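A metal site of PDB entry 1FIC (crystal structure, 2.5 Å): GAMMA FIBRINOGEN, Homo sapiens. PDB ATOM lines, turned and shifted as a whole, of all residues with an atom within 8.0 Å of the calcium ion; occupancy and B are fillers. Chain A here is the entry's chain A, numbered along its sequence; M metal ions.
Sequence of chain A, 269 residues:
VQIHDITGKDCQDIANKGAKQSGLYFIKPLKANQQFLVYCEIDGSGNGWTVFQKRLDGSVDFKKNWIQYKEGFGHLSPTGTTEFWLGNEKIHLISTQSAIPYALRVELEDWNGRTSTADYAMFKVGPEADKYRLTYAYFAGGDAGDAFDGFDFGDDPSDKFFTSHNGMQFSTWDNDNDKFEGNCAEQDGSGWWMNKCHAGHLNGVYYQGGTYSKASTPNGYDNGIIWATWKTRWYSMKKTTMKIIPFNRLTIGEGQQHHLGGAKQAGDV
The calcium ion is bound by OD1 of Asp 176 (2.3 Å).
O of Phe 180 binds the calcium ion.
The side-chain carboxylate (OD2) of Asp 176 binds the calcium ion, 2.4 Å away.
O of Gly 182 is bound to the calcium ion.
The side-chain carboxylate (OD1) of Asp 178 binds the calcium ion (2.6 Å).
OD1 of Asn 183 sits close to OD2 of Asp 176 (3.2 Å).
The side-chain carboxylate (OD2) of Asp 178 lies within hydrogen-bond range of the backbone NH (N) of Cys 184, at 2.9 Å.
The side-chain hydroxyl (OG) of Ser 171 lies within hydrogen-bond range of the backbone NH (N) of Asp 178 (3.3 Å).
O of Glu 181 touches the calcium ion, 3.8 Å away.
Five residues have an atom within 4 Å of the calcium ion: Asp 176, Asp 178, Phe 180, Glu 181 and Gly 182.
The nearest printed residue that does not touch the calcium ion is Asn 183 (4.6 Å).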
ATOM      1  N   SER A 171      11.338 -29.114  10.258  1.00  0.00           N
ATOM      2  CA  SER A 171      11.980 -28.157  11.144  1.00  0.00           C
ATOM      3  C   SER A 171      11.326 -28.169  12.516  1.00  0.00           C
ATOM      4  O   SER A 171      10.105 -28.362  12.652  1.00  0.00           O
ATOM      5  CB  SER A 171      11.882 -26.729  10.596  1.00  0.00           C
ATOM      6  OG  SER A 171      12.424 -26.621   9.283  1.00  0.00           O
ATOM      7  N   ASN A 175      16.140 -27.141  15.371  1.00  0.00           N
ATOM      8  CA  ASN A 175      16.678 -27.677  14.117  1.00  0.00           C
ATOM      9  C   ASN A 175      15.910 -26.989  12.992  1.00  0.00           C
ATOM     10  O   ASN A 175      14.891 -27.490  12.512  1.00  0.00           O
ATOM     11  CB  ASN A 175      16.444 -29.192  14.068  1.00  0.00           C
ATOM     12  CG  ASN A 175      17.323 -29.904  13.054  1.00  0.00           C
ATOM     13  OD1 ASN A 175      17.355 -29.548  11.884  1.00  0.00           O
ATOM     14  ND2 ASN A 175      18.031 -30.917  13.508  1.00  0.00           N
ATOM     15  N   ASP A 176      16.378 -25.799  12.643  1.00  0.00           N
ATOM     16  CA  ASP A 176      15.797 -24.965  11.600  1.00  0.00           C
ATOM     17  C   ASP A 176      16.309 -25.365  10.219  1.00  0.00           C
ATOM     18  O   ASP A 176      17.468 -25.116   9.872  1.00  0.00           O
ATOM     19  CB  ASP A 176      16.131 -23.495  11.895  1.00  0.00           C
ATOM     20  CG  ASP A 176      15.613 -22.522  10.828  1.00  0.00           C
ATOM     21  OD1 ASP A 176      15.816 -22.725   9.618  1.00  0.00           O
ATOM     22  OD2 ASP A 176      15.036 -21.495  11.214  1.00  0.00           O
ATOM     23  N   ASN A 177      15.403 -25.913   9.406  1.00  0.00           N
ATOM     24  CA  ASN A 177      15.700 -26.315   8.034  1.00  0.00           C
ATOM     25  C   ASN A 177      14.752 -25.631   7.045  1.00  0.00           C
ATOM     26  O   ASN A 177      14.540 -26.126   5.928  1.00  0.00           O
ATOM     27  CB  ASN A 177      15.545 -27.819   7.886  1.00  0.00           C
ATOM     28  CG  ASN A 177      16.520 -28.591   8.730  1.00  0.00           C
ATOM     29  OD1 ASN A 177      17.736 -28.483   8.540  1.00  0.00           O
ATOM     30  ND2 ASN A 177      16.002 -29.365   9.665  1.00  0.00           N
ATOM     31  N   ASP A 178      14.153 -24.498   7.458  1.00  0.00           N
ATOM     32  CA  ASP A 178      13.226 -23.766   6.611  1.00  0.00           C
ATOM     33  C   ASP A 178      13.919 -22.796   5.686  1.00  0.00           C
ATOM     34  O   ASP A 178      15.132 -22.567   5.811  1.00  0.00           O
ATOM     35  CB  ASP A 178      12.100 -23.102   7.426  1.00  0.00           C
ATOM     36  CG  ASP A 178      12.574 -21.972   8.331  1.00  0.00           C
ATOM     37  OD1 ASP A 178      13.603 -21.325   8.052  1.00  0.00           O
ATOM     38  OD2 ASP A 178      11.869 -21.681   9.319  1.00  0.00           O
ATOM     39  N   LYS A 179      13.147 -22.226   4.762  1.00  0.00           N
ATOM     40  CA  LYS A 179      13.656 -21.286   3.765  1.00  0.00           C
ATOM     41  C   LYS A 179      13.471 -19.849   4.276  1.00  0.00           C
ATOM     42  O   LYS A 179      13.379 -18.892   3.504  1.00  0.00           O
ATOM     43  CB  LYS A 179      12.900 -21.500   2.446  1.00  0.00           C
ATOM     44  CG  LYS A 179      13.026 -22.911   1.878  1.00  0.00           C
ATOM     45  CD  LYS A 179      14.499 -23.307   1.712  1.00  0.00           C
ATOM     46  CE  LYS A 179      14.710 -24.471   0.730  1.00  0.00           C
ATOM     47  NZ  LYS A 179      14.178 -25.799   1.177  1.00  0.00           N
ATOM     48  N   PHE A 180      13.527 -19.689   5.587  1.00  0.00           N
ATOM     49  CA  PHE A 180      13.306 -18.408   6.207  1.00  0.00           C
ATOM     50  C   PHE A 180      14.528 -17.998   7.020  1.00  0.00           C
ATOM     51  O   PHE A 180      15.143 -18.831   7.689  1.00  0.00           O
ATOM     52  CB  PHE A 180      12.087 -18.551   7.127  1.00  0.00           C
ATOM     53  CG  PHE A 180      11.783 -17.364   7.975  1.00  0.00           C
ATOM     54  CD1 PHE A 180      11.767 -16.089   7.441  1.00  0.00           C
ATOM     55  CD2 PHE A 180      11.443 -17.535   9.308  1.00  0.00           C
ATOM     56  CE1 PHE A 180      11.403 -14.988   8.208  1.00  0.00           C
ATOM     57  CE2 PHE A 180      11.071 -16.442  10.095  1.00  0.00           C
ATOM     58  CZ  PHE A 180      11.056 -15.165   9.546  1.00  0.00           C
ATOM     59  N   GLU A 181      14.839 -16.700   6.960  1.00  0.00           N
ATOM     60  CA  GLU A 181      15.965 -16.126   7.704  1.00  0.00           C
ATOM     61  C   GLU A 181      15.838 -16.518   9.163  1.00  0.00           C
ATOM     62  O   GLU A 181      16.823 -16.863   9.811  1.00  0.00           O
ATOM     63  CB  GLU A 181      15.957 -14.599   7.603  1.00  0.00           C
ATOM     64  CG  GLU A 181      16.025 -14.043   6.186  1.00  0.00           C
ATOM     65  CD  GLU A 181      14.670 -13.985   5.470  1.00  0.00           C
ATOM     66  OE1 GLU A 181      13.764 -13.276   5.966  1.00  0.00           O
ATOM     67  OE2 GLU A 181      14.513 -14.635   4.406  1.00  0.00           O
ATOM     68  N   GLY A 182      14.616 -16.422   9.689  1.00  0.00           N
ATOM     69  CA  GLY A 182      14.355 -16.768  11.081  1.00  0.00           C
ATOM     70  C   GLY A 182      13.977 -18.223  11.270  1.00  0.00           C
ATOM     71  O   GLY A 182      14.379 -19.090  10.487  1.00  0.00           O
ATOM     72  N   ASN A 183      13.146 -18.487  12.287  1.00  0.00           N
ATOM     73  CA  ASN A 183      12.731 -19.847  12.600  1.00  0.00           C
ATOM     74  C   ASN A 183      11.212 -19.984  12.691  1.00  0.00           C
ATOM     75  O   ASN A 183      10.605 -19.689  13.739  1.00  0.00           O
ATOM     76  CB  ASN A 183      13.378 -20.298  13.913  1.00  0.00           C
ATOM     77  CG  ASN A 183      13.525 -21.820  14.012  1.00  0.00           C
ATOM     78  OD1 ASN A 183      12.844 -22.591  13.320  1.00  0.00           O
ATOM     79  ND2 ASN A 183      14.446 -22.255  14.875  1.00  0.00           N
ATOM     80  N   CYS A 184      10.596 -20.450  11.602  1.00  0.00           N
ATOM     81  CA  CYS A 184       9.157 -20.652  11.594  1.00  0.00           C
ATOM     82  C   CYS A 184       8.762 -21.588  12.739  1.00  0.00           C
ATOM     83  O   CYS A 184       7.802 -21.330  13.466  1.00  0.00           O
ATOM     84  CB  CYS A 184       8.723 -21.263  10.260  1.00  0.00           C
ATOM     85  SG  CYS A 184       8.955 -20.219   8.789  1.00  0.00           S
ATOM     86  N   ALA A 185       9.531 -22.657  12.919  1.00  0.00           N
ATOM     87  CA  ALA A 185       9.254 -23.662  13.931  1.00  0.00           C
ATOM     88  C   ALA A 185       9.305 -23.098  15.330  1.00  0.00           C
ATOM     89  O   ALA A 185       8.395 -23.332  16.129  1.00  0.00           O
ATOM     90  CB  ALA A 185      10.209 -24.800  13.802  1.00  0.00           C
ATOM     91  N   ASN A 195       8.327 -23.608   5.115  1.00  0.00           N
ATOM     92  CA  ASN A 195       8.933 -22.964   3.952  1.00  0.00           C
ATOM     93  C   ASN A 195       9.320 -21.562   4.491  1.00  0.00           C
ATOM     94  O   ASN A 195      10.092 -21.479   5.467  1.00  0.00           O
ATOM     95  CB  ASN A 195       7.897 -22.875   2.835  1.00  0.00           C
ATOM     96  CG  ASN A 195       8.482 -22.370   1.548  1.00  0.00           C
ATOM     97  OD1 ASN A 195       9.555 -21.764   1.547  1.00  0.00           O
ATOM     98  ND2 ASN A 195       7.800 -22.632   0.443  1.00  0.00           N
HETATM   99 CA    CA M   1      15.823 -20.517   9.149  1.00  0.00          CA
